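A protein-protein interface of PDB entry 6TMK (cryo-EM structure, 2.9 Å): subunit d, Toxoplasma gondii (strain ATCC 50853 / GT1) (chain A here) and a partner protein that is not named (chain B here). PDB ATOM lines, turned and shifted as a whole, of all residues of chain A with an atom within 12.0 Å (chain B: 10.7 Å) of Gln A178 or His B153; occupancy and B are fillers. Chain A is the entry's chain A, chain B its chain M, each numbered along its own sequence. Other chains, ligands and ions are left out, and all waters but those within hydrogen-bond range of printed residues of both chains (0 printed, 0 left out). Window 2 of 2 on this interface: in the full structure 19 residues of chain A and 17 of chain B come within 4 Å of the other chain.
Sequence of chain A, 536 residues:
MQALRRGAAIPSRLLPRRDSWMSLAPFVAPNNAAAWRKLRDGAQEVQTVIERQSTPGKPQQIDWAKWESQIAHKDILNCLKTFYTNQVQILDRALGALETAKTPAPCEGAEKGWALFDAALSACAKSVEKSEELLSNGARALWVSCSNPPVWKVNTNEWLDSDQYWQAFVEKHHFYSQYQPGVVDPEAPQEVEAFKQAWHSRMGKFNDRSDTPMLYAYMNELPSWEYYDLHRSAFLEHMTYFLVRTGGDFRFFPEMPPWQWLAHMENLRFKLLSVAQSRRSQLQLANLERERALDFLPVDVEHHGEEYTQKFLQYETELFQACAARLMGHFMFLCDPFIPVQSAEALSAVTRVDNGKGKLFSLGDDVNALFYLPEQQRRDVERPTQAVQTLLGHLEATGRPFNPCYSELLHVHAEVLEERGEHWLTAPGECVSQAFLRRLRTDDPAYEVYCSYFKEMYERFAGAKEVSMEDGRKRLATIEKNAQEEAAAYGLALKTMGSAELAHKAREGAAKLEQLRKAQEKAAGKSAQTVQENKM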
ATOM      1  N   PHE A 169       8.980 -31.165 -21.585  1.00  0.00           N
ATOM      2  CA  PHE A 169      10.184 -31.493 -20.839  1.00  0.00           C
ATOM      3  C   PHE A 169      11.383 -30.718 -21.368  1.00  0.00           C
ATOM      4  O   PHE A 169      12.252 -30.299 -20.596  1.00  0.00           O
ATOM      5  CB  PHE A 169      10.406 -32.999 -20.906  1.00  0.00           C
ATOM      6  CG  PHE A 169      11.408 -33.515 -19.930  1.00  0.00           C
ATOM      7  CD1 PHE A 169      11.065 -33.717 -18.613  1.00  0.00           C
ATOM      8  CD2 PHE A 169      12.683 -33.833 -20.334  1.00  0.00           C
ATOM      9  CE1 PHE A 169      11.978 -34.197 -17.721  1.00  0.00           C
ATOM     10  CE2 PHE A 169      13.597 -34.315 -19.443  1.00  0.00           C
ATOM     11  CZ  PHE A 169      13.243 -34.503 -18.137  1.00  0.00           C
ATOM     12  N   VAL A 170      11.442 -30.516 -22.683  1.00  0.00           N
ATOM     13  CA  VAL A 170      12.549 -29.797 -23.295  1.00  0.00           C
ATOM     14  C   VAL A 170      12.429 -28.300 -23.051  1.00  0.00           C
ATOM     15  O   VAL A 170      13.421 -27.625 -22.764  1.00  0.00           O
ATOM     16  CB  VAL A 170      12.576 -30.133 -24.799  1.00  0.00           C
ATOM     17  CG1 VAL A 170      13.513 -29.226 -25.562  1.00  0.00           C
ATOM     18  CG2 VAL A 170      12.948 -31.569 -24.995  1.00  0.00           C
ATOM     19  N   GLU A 171      11.219 -27.761 -23.176  1.00  0.00           N
ATOM     20  CA  GLU A 171      10.987 -26.345 -22.915  1.00  0.00           C
ATOM     21  C   GLU A 171      11.371 -25.971 -21.487  1.00  0.00           C
ATOM     22  O   GLU A 171      11.930 -24.894 -21.238  1.00  0.00           O
ATOM     23  CB  GLU A 171       9.520 -26.033 -23.186  1.00  0.00           C
ATOM     24  CG  GLU A 171       9.207 -24.617 -23.569  1.00  0.00           C
ATOM     25  CD  GLU A 171       7.722 -24.334 -23.533  1.00  0.00           C
ATOM     26  OE1 GLU A 171       6.951 -25.258 -23.198  1.00  0.00           O
ATOM     27  OE2 GLU A 171       7.322 -23.194 -23.844  1.00  0.00           O
ATOM     28  N   LYS A 172      11.075 -26.860 -20.539  1.00  0.00           N
ATOM     29  CA  LYS A 172      11.321 -26.591 -19.129  1.00  0.00           C
ATOM     30  C   LYS A 172      12.796 -26.371 -18.835  1.00  0.00           C
ATOM     31  O   LYS A 172      13.154 -25.511 -18.024  1.00  0.00           O
ATOM     32  CB  LYS A 172      10.780 -27.746 -18.300  1.00  0.00           C
ATOM     33  CG  LYS A 172      10.698 -27.477 -16.830  1.00  0.00           C
ATOM     34  CD  LYS A 172      10.701 -28.752 -16.047  1.00  0.00           C
ATOM     35  CE  LYS A 172      10.972 -28.497 -14.594  1.00  0.00           C
ATOM     36  NZ  LYS A 172      10.154 -29.355 -13.720  1.00  0.00           N
ATOM     37  N   HIS A 173      13.665 -27.135 -19.482  1.00  0.00           N
ATOM     38  CA  HIS A 173      15.078 -27.159 -19.142  1.00  0.00           C
ATOM     39  C   HIS A 173      15.952 -26.392 -20.117  1.00  0.00           C
ATOM     40  O   HIS A 173      17.071 -26.017 -19.751  1.00  0.00           O
ATOM     41  CB  HIS A 173      15.568 -28.606 -19.054  1.00  0.00           C
ATOM     42  CG  HIS A 173      14.963 -29.374 -17.926  1.00  0.00           C
ATOM     43  ND1 HIS A 173      15.308 -29.152 -16.612  1.00  0.00           N
ATOM     44  CD2 HIS A 173      14.023 -30.346 -17.910  1.00  0.00           C
ATOM     45  CE1 HIS A 173      14.614 -29.962 -15.836  1.00  0.00           C
ATOM     46  NE2 HIS A 173      13.825 -30.695 -16.599  1.00  0.00           N
ATOM     47  N   HIS A 174      15.480 -26.153 -21.331  1.00  0.00           N
ATOM     48  CA  HIS A 174      16.301 -25.583 -22.380  1.00  0.00           C
ATOM     49  C   HIS A 174      15.726 -24.315 -22.985  1.00  0.00           C
ATOM     50  O   HIS A 174      16.446 -23.616 -23.705  1.00  0.00           O
ATOM     51  CB  HIS A 174      16.540 -26.630 -23.470  1.00  0.00           C
ATOM     52  CG  HIS A 174      17.314 -27.808 -22.982  1.00  0.00           C
ATOM     53  ND1 HIS A 174      16.788 -29.079 -22.933  1.00  0.00           N
ATOM     54  CD2 HIS A 174      18.563 -27.897 -22.469  1.00  0.00           C
ATOM     55  CE1 HIS A 174      17.690 -29.905 -22.437  1.00  0.00           C
ATOM     56  NE2 HIS A 174      18.775 -29.212 -22.148  1.00  0.00           N
ATOM     57  N   PHE A 175      14.466 -23.997 -22.711  1.00  0.00           N
ATOM     58  CA  PHE A 175      13.882 -22.707 -23.044  1.00  0.00           C
ATOM     59  C   PHE A 175      13.764 -21.802 -21.834  1.00  0.00           C
ATOM     60  O   PHE A 175      14.026 -20.603 -21.935  1.00  0.00           O
ATOM     61  CB  PHE A 175      12.500 -22.890 -23.666  1.00  0.00           C
ATOM     62  CG  PHE A 175      11.724 -21.621 -23.792  1.00  0.00           C
ATOM     63  CD1 PHE A 175      12.071 -20.675 -24.727  1.00  0.00           C
ATOM     64  CD2 PHE A 175      10.646 -21.373 -22.975  1.00  0.00           C
ATOM     65  CE1 PHE A 175      11.358 -19.514 -24.840  1.00  0.00           C
ATOM     66  CE2 PHE A 175       9.937 -20.213 -23.087  1.00  0.00           C
ATOM     67  CZ  PHE A 175      10.291 -19.283 -24.020  1.00  0.00           C
ATOM     68  N   TYR A 176      13.386 -22.351 -20.686  1.00  0.00           N
ATOM     69  CA  TYR A 176      13.299 -21.544 -19.480  1.00  0.00           C
ATOM     70  C   TYR A 176      14.644 -21.382 -18.790  1.00  0.00           C
ATOM     71  O   TYR A 176      14.774 -20.522 -17.915  1.00  0.00           O
ATOM     72  CB  TYR A 176      12.279 -22.153 -18.529  1.00  0.00           C
ATOM     73  CG  TYR A 176      10.859 -21.952 -18.989  1.00  0.00           C
ATOM     74  CD1 TYR A 176      10.246 -20.722 -18.879  1.00  0.00           C
ATOM     75  CD2 TYR A 176      10.139 -22.988 -19.551  1.00  0.00           C
ATOM     76  CE1 TYR A 176       8.960 -20.531 -19.304  1.00  0.00           C
ATOM     77  CE2 TYR A 176       8.852 -22.805 -19.977  1.00  0.00           C
ATOM     78  CZ  TYR A 176       8.266 -21.575 -19.856  1.00  0.00           C
ATOM     79  OH  TYR A 176       6.976 -21.394 -20.283  1.00  0.00           O
ATOM     80  N   SER A 177      15.639 -22.179 -19.166  1.00  0.00           N
ATOM     81  CA  SER A 177      17.006 -22.013 -18.706  1.00  0.00           C
ATOM     82  C   SER A 177      17.948 -22.062 -19.899  1.00  0.00           C
ATOM     83  O   SER A 177      17.589 -22.511 -20.989  1.00  0.00           O
ATOM     84  CB  SER A 177      17.400 -23.084 -17.692  1.00  0.00           C
ATOM     85  OG  SER A 177      18.600 -22.734 -17.029  1.00  0.00           O
ATOM     86  N   GLN A 178      19.172 -21.593 -19.670  1.00  0.00           N
ATOM     87  CA  GLN A 178      20.222 -21.585 -20.675  1.00  0.00           C
ATOM     88  C   GLN A 178      21.463 -22.338 -20.230  1.00  0.00           C
ATOM     89  O   GLN A 178      22.397 -22.484 -21.025  1.00  0.00           O
ATOM     90  CB  GLN A 178      20.621 -20.149 -21.034  1.00  0.00           C
ATOM     91  CG  GLN A 178      19.546 -19.301 -21.675  1.00  0.00           C
ATOM     92  CD  GLN A 178      19.344 -19.614 -23.135  1.00  0.00           C
ATOM     93  OE1 GLN A 178      18.237 -19.924 -23.568  1.00  0.00           O
ATOM     94  NE2 GLN A 178      20.419 -19.544 -23.906  1.00  0.00           N
ATOM     95  N   TYR A 179      21.500 -22.825 -18.993  1.00  0.00           N
ATOM     96  CA  TYR A 179      22.697 -23.425 -18.423  1.00  0.00           C
ATOM     97  C   TYR A 179      22.486 -24.866 -17.984  1.00  0.00           C
ATOM     98  O   TYR A 179      23.359 -25.433 -17.319  1.00  0.00           O
ATOM     99  CB  TYR A 179      23.186 -22.585 -17.243  1.00  0.00           C
ATOM    100  CG  TYR A 179      23.542 -21.171 -17.607  1.00  0.00           C
ATOM    101  CD1 TYR A 179      24.594 -20.901 -18.460  1.00  0.00           C
ATOM    102  CD2 TYR A 179      22.827 -20.106 -17.100  1.00  0.00           C
ATOM    103  CE1 TYR A 179      24.923 -19.612 -18.791  1.00  0.00           C
ATOM    104  CE2 TYR A 179      23.151 -18.820 -17.424  1.00  0.00           C
ATOM    105  CZ  TYR A 179      24.195 -18.572 -18.272  1.00  0.00           C
ATOM    106  OH  TYR A 179      24.514 -17.276 -18.597  1.00  0.00           O
ATOM    107  N   GLN A 180      21.366 -25.467 -18.325  1.00  0.00           N
ATOM    108  CA  GLN A 180      21.122 -26.841 -17.938  1.00  0.00           C
ATOM    109  C   GLN A 180      21.931 -27.783 -18.825  1.00  0.00           C
ATOM    110  O   GLN A 180      22.129 -27.511 -20.011  1.00  0.00           O
ATOM    111  CB  GLN A 180      19.643 -27.174 -18.047  1.00  0.00           C
ATOM    112  CG  GLN A 180      18.784 -26.558 -16.974  1.00  0.00           C
ATOM    113  CD  GLN A 180      19.009 -27.186 -15.628  1.00  0.00           C
ATOM    114  OE1 GLN A 180      19.938 -26.830 -14.906  1.00  0.00           O
ATOM    115  NE2 GLN A 180      18.162 -28.137 -15.281  1.00  0.00           N
ATOM    116  N   PRO A 181      22.402 -28.900 -18.281  1.00  0.00           N
ATOM    117  CA  PRO A 181      23.239 -29.798 -19.076  1.00  0.00           C
ATOM    118  C   PRO A 181      22.447 -30.509 -20.156  1.00  0.00           C
ATOM    119  O   PRO A 181      21.241 -30.736 -20.035  1.00  0.00           O
ATOM    120  CB  PRO A 181      23.773 -30.787 -18.038  1.00  0.00           C
ATOM    121  CG  PRO A 181      22.737 -30.800 -16.990  1.00  0.00           C
ATOM    122  CD  PRO A 181      22.220 -29.405 -16.912  1.00  0.00           C
ATOM    123  N   GLY A 182      23.148 -30.863 -21.226  1.00  0.00           N
ATOM    124  CA  GLY A 182      22.513 -31.552 -22.326  1.00  0.00           C
ATOM    125  C   GLY A 182      22.458 -33.046 -22.117  1.00  0.00           C
ATOM    126  O   GLY A 182      22.963 -33.816 -22.937  1.00  0.00           O
ATOM    127  N   VAL A 183      21.835 -33.466 -21.024  1.00  0.00           N
ATOM    128  CA  VAL A 183      21.696 -34.877 -20.711  1.00  0.00           C
ATOM    129  C   VAL A 183      20.233 -35.254 -20.873  1.00  0.00           C
ATOM    130  O   VAL A 183      19.337 -34.406 -20.891  1.00  0.00           O
ATOM    131  CB  VAL A 183      22.208 -35.220 -19.297  1.00  0.00           C
ATOM    132  CG1 VAL A 183      23.693 -34.992 -19.213  1.00  0.00           C
ATOM    133  CG2 VAL A 183      21.491 -34.404 -18.247  1.00  0.00           C
ATOM    134  N   PRO A 186      17.779 -34.320 -16.869  1.00  0.00           N
ATOM    135  CA  PRO A 186      18.348 -33.343 -15.934  1.00  0.00           C
ATOM    136  C   PRO A 186      17.675 -33.317 -14.575  1.00  0.00           C
ATOM    137  O   PRO A 186      18.239 -32.729 -13.642  1.00  0.00           O
ATOM    138  CB  PRO A 186      18.150 -32.008 -16.661  1.00  0.00           C
ATOM    139  CG  PRO A 186      17.764 -32.341 -18.036  1.00  0.00           C
ATOM    140  CD  PRO A 186      17.113 -33.665 -17.998  1.00  0.00           C
ATOM    141  N   PHE A 195      24.062 -30.812  -8.249  1.00  0.00           N
ATOM    142  CA  PHE A 195      23.773 -29.387  -8.161  1.00  0.00           C
ATOM    143  C   PHE A 195      23.841 -28.906  -6.722  1.00  0.00           C
ATOM    144  O   PHE A 195      24.384 -27.832  -6.444  1.00  0.00           O
ATOM    145  CB  PHE A 195      22.398 -29.100  -8.754  1.00  0.00           C
ATOM    146  CG  PHE A 195      22.069 -27.640  -8.840  1.00  0.00           C
ATOM    147  CD1 PHE A 195      22.502 -26.885  -9.909  1.00  0.00           C
ATOM    148  CD2 PHE A 195      21.325 -27.023  -7.853  1.00  0.00           C
ATOM    149  CE1 PHE A 195      22.201 -25.547  -9.992  1.00  0.00           C
ATOM    150  CE2 PHE A 195      21.026 -25.686  -7.933  1.00  0.00           C
ATOM    151  CZ  PHE A 195      21.462 -24.948  -9.003  1.00  0.00           C
ATOM    152  N   LEU B 145      31.075 -14.628 -32.203  1.00  0.00           N
ATOM    153  CA  LEU B 145      31.003 -15.261 -30.892  1.00  0.00           C
ATOM    154  C   LEU B 145      29.557 -15.545 -30.516  1.00  0.00           C
ATOM    155  O   LEU B 145      29.226 -16.632 -30.024  1.00  0.00           O
ATOM    156  CB  LEU B 145      31.655 -14.374 -29.837  1.00  0.00           C
ATOM    157  CG  LEU B 145      33.160 -14.162 -29.931  1.00  0.00           C
ATOM    158  CD1 LEU B 145      33.627 -13.277 -28.809  1.00  0.00           C
ATOM    159  CD2 LEU B 145      33.877 -15.478 -29.878  1.00  0.00           C
ATOM    160  N   ALA B 146      28.681 -14.565 -30.730  1.00  0.00           N
ATOM    161  CA  ALA B 146      27.262 -14.793 -30.477  1.00  0.00           C
ATOM    162  C   ALA B 146      26.727 -15.944 -31.322  1.00  0.00           C
ATOM    163  O   ALA B 146      25.985 -16.805 -30.829  1.00  0.00           O
ATOM    164  CB  ALA B 146      26.475 -13.520 -30.762  1.00  0.00           C
ATOM    165  N   TYR B 147      27.090 -15.961 -32.603  1.00  0.00           N
ATOM    166  CA  TYR B 147      26.671 -17.019 -33.513  1.00  0.00           C
ATOM    167  C   TYR B 147      27.103 -18.389 -33.012  1.00  0.00           C
ATOM    168  O   TYR B 147      26.321 -19.346 -33.030  1.00  0.00           O
ATOM    169  CB  TYR B 147      27.263 -16.724 -34.891  1.00  0.00           C
ATOM    170  CG  TYR B 147      27.106 -17.783 -35.948  1.00  0.00           C
ATOM    171  CD1 TYR B 147      26.055 -17.741 -36.842  1.00  0.00           C
ATOM    172  CD2 TYR B 147      28.037 -18.799 -36.084  1.00  0.00           C
ATOM    173  CE1 TYR B 147      25.922 -18.687 -37.819  1.00  0.00           C
ATOM    174  CE2 TYR B 147      27.907 -19.751 -37.054  1.00  0.00           C
ATOM    175  CZ  TYR B 147      26.850 -19.694 -37.920  1.00  0.00           C
ATOM    176  OH  TYR B 147      26.726 -20.647 -38.897  1.00  0.00           O
ATOM    177  N   LEU B 148      28.350 -18.503 -32.561  1.00  0.00           N
ATOM    178  CA  LEU B 148      28.861 -19.791 -32.111  1.00  0.00           C
ATOM    179  C   LEU B 148      28.202 -20.225 -30.812  1.00  0.00           C
ATOM    180  O   LEU B 148      27.938 -21.414 -30.613  1.00  0.00           O
ATOM    181  CB  LEU B 148      30.377 -19.732 -31.950  1.00  0.00           C
ATOM    182  CG  LEU B 148      31.178 -19.610 -33.243  1.00  0.00           C
ATOM    183  CD1 LEU B 148      32.646 -19.437 -32.944  1.00  0.00           C
ATOM    184  CD2 LEU B 148      30.952 -20.812 -34.132  1.00  0.00           C
ATOM    185  N   ALA B 149      27.928 -19.282 -29.915  1.00  0.00           N
ATOM    186  CA  ALA B 149      27.231 -19.628 -28.683  1.00  0.00           C
ATOM    187  C   ALA B 149      25.836 -20.160 -28.981  1.00  0.00           C
ATOM    188  O   ALA B 149      25.407 -21.175 -28.419  1.00  0.00           O
ATOM    189  CB  ALA B 149      27.164 -18.414 -27.762  1.00  0.00           C
ATOM    190  N   MET B 150      25.116 -19.480 -29.872  1.00  0.00           N
ATOM    191  CA  MET B 150      23.789 -19.934 -30.271  1.00  0.00           C
ATOM    192  C   MET B 150      23.852 -21.318 -30.907  1.00  0.00           C
ATOM    193  O   MET B 150      23.035 -22.200 -30.605  1.00  0.00           O
ATOM    194  CB  MET B 150      23.190 -18.914 -31.231  1.00  0.00           C
ATOM    195  CG  MET B 150      21.717 -19.026 -31.454  1.00  0.00           C
ATOM    196  SD  MET B 150      20.984 -17.414 -31.731  1.00  0.00           S
ATOM    197  CE  MET B 150      19.274 -17.888 -31.849  1.00  0.00           C
ATOM    198  N   LEU B 151      24.806 -21.512 -31.817  1.00  0.00           N
ATOM    199  CA  LEU B 151      24.992 -22.804 -32.460  1.00  0.00           C
ATOM    200  C   LEU B 151      25.249 -23.903 -31.438  1.00  0.00           C
ATOM    201  O   LEU B 151      24.686 -24.999 -31.539  1.00  0.00           O
ATOM    202  CB  LEU B 151      26.151 -22.702 -33.443  1.00  0.00           C
ATOM    203  CG  LEU B 151      26.375 -23.822 -34.447  1.00  0.00           C
ATOM    204  CD1 LEU B 151      25.354 -23.745 -35.550  1.00  0.00           C
ATOM    205  CD2 LEU B 151      27.766 -23.712 -34.997  1.00  0.00           C
ATOM    206  N   GLY B 152      26.097 -23.632 -30.447  1.00  0.00           N
ATOM    207  CA  GLY B 152      26.395 -24.636 -29.443  1.00  0.00           C
ATOM    208  C   GLY B 152      25.200 -24.956 -28.571  1.00  0.00           C
ATOM    209  O   GLY B 152      24.982 -26.110 -28.196  1.00  0.00           O
ATOM    210  N   HIS B 153      24.408 -23.940 -28.238  1.00  0.00           N
ATOM    211  CA  HIS B 153      23.187 -24.170 -27.476  1.00  0.00           C
ATOM    212  C   HIS B 153      22.234 -25.081 -28.234  1.00  0.00           C
ATOM    213  O   HIS B 153      21.707 -26.061 -27.685  1.00  0.00           O
ATOM    214  CB  HIS B 153      22.507 -22.844 -27.167  1.00  0.00           C
ATOM    215  CG  HIS B 153      21.398 -22.958 -26.175  1.00  0.00           C
ATOM    216  ND1 HIS B 153      21.580 -23.481 -24.914  1.00  0.00           N
ATOM    217  CD2 HIS B 153      20.087 -22.646 -26.268  1.00  0.00           C
ATOM    218  CE1 HIS B 153      20.430 -23.469 -24.267  1.00  0.00           C
ATOM    219  NE2 HIS B 153      19.508 -22.966 -25.066  1.00  0.00           N
ATOM    220  N   GLU B 154      21.996 -24.768 -29.505  1.00  0.00           N
ATOM    221  CA  GLU B 154      21.090 -25.588 -30.292  1.00  0.00           C
ATOM    222  C   GLU B 154      21.643 -26.989 -30.501  1.00  0.00           C
ATOM    223  O   GLU B 154      20.873 -27.952 -30.542  1.00  0.00           O
ATOM    224  CB  GLU B 154      20.804 -24.908 -31.625  1.00  0.00           C
ATOM    225  CG  GLU B 154      20.029 -23.617 -31.484  1.00  0.00           C
ATOM    226  CD  GLU B 154      19.252 -23.254 -32.728  1.00  0.00           C
ATOM    227  OE1 GLU B 154      18.479 -22.276 -32.678  1.00  0.00           O
ATOM    228  OE2 GLU B 154      19.412 -23.942 -33.757  1.00  0.00           O
ATOM    229  N   GLY B 155      22.964 -27.135 -30.609  1.00  0.00           N
ATOM    230  CA  GLY B 155      23.545 -28.462 -30.696  1.00  0.00           C
ATOM    231  C   GLY B 155      23.353 -29.266 -29.424  1.00  0.00           C
ATOM    232  O   GLY B 155      23.093 -30.472 -29.471  1.00  0.00           O
ATOM    233  N   LYS B 156      23.501 -28.614 -28.273  1.00  0.00           N
ATOM    234  CA  LYS B 156      23.214 -29.262 -27.000  1.00  0.00           C
ATOM    235  C   LYS B 156      21.781 -29.767 -26.956  1.00  0.00           C
ATOM    236  O   LYS B 156      21.518 -30.908 -26.553  1.00  0.00           O
ATOM    237  CB  LYS B 156      23.471 -28.278 -25.864  1.00  0.00           C
ATOM    238  CG  LYS B 156      23.399 -28.875 -24.495  1.00  0.00           C
ATOM    239  CD  LYS B 156      23.781 -27.881 -23.449  1.00  0.00           C
ATOM    240  CE  LYS B 156      22.661 -26.921 -23.182  1.00  0.00           C
ATOM    241  NZ  LYS B 156      22.922 -26.088 -21.983  1.00  0.00           N
ATOM    242  N   ILE B 157      20.837 -28.920 -27.361  1.00  0.00           N
ATOM    243  CA  ILE B 157      19.433 -29.319 -27.352  1.00  0.00           C
ATOM    244  C   ILE B 157      19.206 -30.478 -28.312  1.00  0.00           C
ATOM    245  O   ILE B 157      18.445 -31.410 -28.022  1.00  0.00           O
ATOM    246  CB  ILE B 157      18.536 -28.118 -27.694  1.00  0.00           C
ATOM    247  CG1 ILE B 157      18.671 -27.032 -26.638  1.00  0.00           C
ATOM    248  CG2 ILE B 157      17.107 -28.546 -27.787  1.00  0.00           C
ATOM    249  CD1 ILE B 157      18.296 -25.686 -27.125  1.00  0.00           C
ATOM    250  N   HIS B 158      19.850 -30.431 -29.477  1.00  0.00           N
ATOM    251  CA  HIS B 158      19.732 -31.504 -30.453  1.00  0.00           C
ATOM    252  C   HIS B 158      20.192 -32.827 -29.864  1.00  0.00           C
ATOM    253  O   HIS B 158      19.511 -33.847 -29.994  1.00  0.00           O
ATOM    254  CB  HIS B 158      20.543 -31.161 -31.698  1.00  0.00           C
ATOM    255  CG  HIS B 158      20.199 -31.992 -32.891  1.00  0.00           C
ATOM    256  ND1 HIS B 158      20.268 -33.366 -32.886  1.00  0.00           N
ATOM    257  CD2 HIS B 158      19.797 -31.640 -34.134  1.00  0.00           C
ATOM    258  CE1 HIS B 158      19.908 -33.827 -34.069  1.00  0.00           C
ATOM    259  NE2 HIS B 158      19.620 -32.799 -34.845  1.00  0.00           N
ATOM    260  N   GLY B 159      21.362 -32.831 -29.228  1.00  0.00           N
ATOM    261  CA  GLY B 159      21.848 -34.051 -28.606  1.00  0.00           C
ATOM    262  C   GLY B 159      20.921 -34.554 -27.519  1.00  0.00           C
ATOM    263  O   GLY B 159      20.662 -35.757 -27.413  1.00  0.00           O
ATOM    264  N   ALA B 160      20.402 -33.640 -26.702  1.00  0.00           N
ATOM    265  CA  ALA B 160      19.498 -34.037 -25.632  1.00  0.00           C
ATOM    266  C   ALA B 160      18.259 -34.719 -26.192  1.00  0.00           C
ATOM    267  O   ALA B 160      17.850 -35.778 -25.706  1.00  0.00           O
ATOM    268  CB  ALA B 160      19.108 -32.823 -24.798  1.00  0.00           C
ATOM    269  N   VAL B 161      17.646 -34.128 -27.215  1.00  0.00           N
ATOM    270  CA  VAL B 161      16.440 -34.719 -27.785  1.00  0.00           C
ATOM    271  C   VAL B 161      16.768 -36.019 -28.505  1.00  0.00           C
ATOM    272  O   VAL B 161      15.973 -36.965 -28.498  1.00  0.00           O
ATOM    273  CB  VAL B 161      15.749 -33.718 -28.726  1.00  0.00           C
ATOM    274  CG1 VAL B 161      14.505 -34.324 -29.316  1.00  0.00           C
ATOM    275  CG2 VAL B 161      15.397 -32.464 -27.994  1.00  0.00           C
ATOM    276  N   ARG B 163      18.970 -38.184 -27.690  1.00  0.00           N
ATOM    277  CA  ARG B 163      19.073 -39.241 -26.691  1.00  0.00           C
ATOM    278  C   ARG B 163      17.722 -39.546 -26.056  1.00  0.00           C
ATOM    279  O   ARG B 163      17.412 -40.712 -25.776  1.00  0.00           O
ATOM    280  CB  ARG B 163      20.087 -38.852 -25.622  1.00  0.00           C
ATOM    281  CG  ARG B 163      21.489 -38.736 -26.150  1.00  0.00           C
ATOM    282  CD  ARG B 163      22.493 -38.376 -25.088  1.00  0.00           C
ATOM    283  NE  ARG B 163      23.824 -38.250 -25.669  1.00  0.00           N
ATOM    284  CZ  ARG B 163      24.391 -37.101 -26.021  1.00  0.00           C
ATOM    285  NH1 ARG B 163      23.763 -35.953 -25.842  1.00  0.00           N
ATOM    286  NH2 ARG B 163      25.596 -37.101 -26.559  1.00  0.00           N
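A ring nitrogen (NE2) of His B153 is in hydrogen-bond range of the backbone carbonyl oxygen (O) of His A174, at 3.4 Å.
The side-chain amino group (NZ) of Lys B156 is in hydrogen-bond range of the backbone carbonyl oxygen (O) of Gln A180 (2.6 Å).
ND1 of His A173 sits at hydrogen-bond distance from NE2 of Gln A180, at 3.3 Å.
The backbone carbonyl oxygen (O) of Gly B159 sits close to the guanidinium group (NH1) of Arg B163 (3.5 Å).
CG2 of Val B161 touches CG2 of Val A170, at 3.97 Å.
Ile B157 touches His A174 (CG1 to CB, 3.8 Å).
His B153 touches Gln A178 (NE2 to OE1, 3.6 Å).
Gln A178 touches Lys B156.
CG of Lys B156 touches CA of Gly A182, 3.6 Å away.
NH1 of Arg B163 touches O of Gly A182 (3.7 Å).
Of chain B, only His B153 (3.6 Å) and Lys B156 (3.8 Å) come within 4 Å of Gln A178.
His B153 touches two residues of chain A.
No residue of chain B comes within 4 Å of Ser A177.
No residue of chain B comes within 4 Å of Tyr A179.
No residue of chain A comes within 4 Å of Ala B149.
No residue of chain A comes within 4 Å of Leu B151.
No residue of chain A comes within 4 Å of Gly B152.
Glu B154 touches none of the printed residues of chain A.
Lys B156 touches just these residues of chain A: Gln A178, Gln A180 and Gly A182.
Ile B157 touches one residue of chain A.
Of the printed residues of chain A, Arg B163 touches Gly A182 (3.7 Å).
Of the printed residues of chain B, Val A170 touches Val B161 (3.97 Å).
Of the printed residues of chain B, His A174 touches His B153 (3.4 Å) and Ile B157 (3.8 Å).
The nearest residue of chain B that does not touch Gln A178 is Ile B157 (6.8 Å).
The nearest residue of chain A that does not touch His B153 is Ser A177 (4.4 Å).
The nearest printed residue of chain B that does not touch His A174 is Ala B160 (4.01 Å).
Printed residues of chain A that touch a printed residue of chain B: Val A170, His A174, Gln A178, Gln A180 and Gly A182.
Hydrophobic or aromatic side chains of chain A within 4 Å of the printed part of chain B: Val A170 and His A174.
Printed residues of chain B that touch a printed residue of chain A: His B153, Lys B156, Ile B157, Val B161 and Arg B163.
Among the printed residues, no Asp or Glu carboxylate lies within 4 Å of a Lys or Arg side-chain nitrogen of the other chain.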
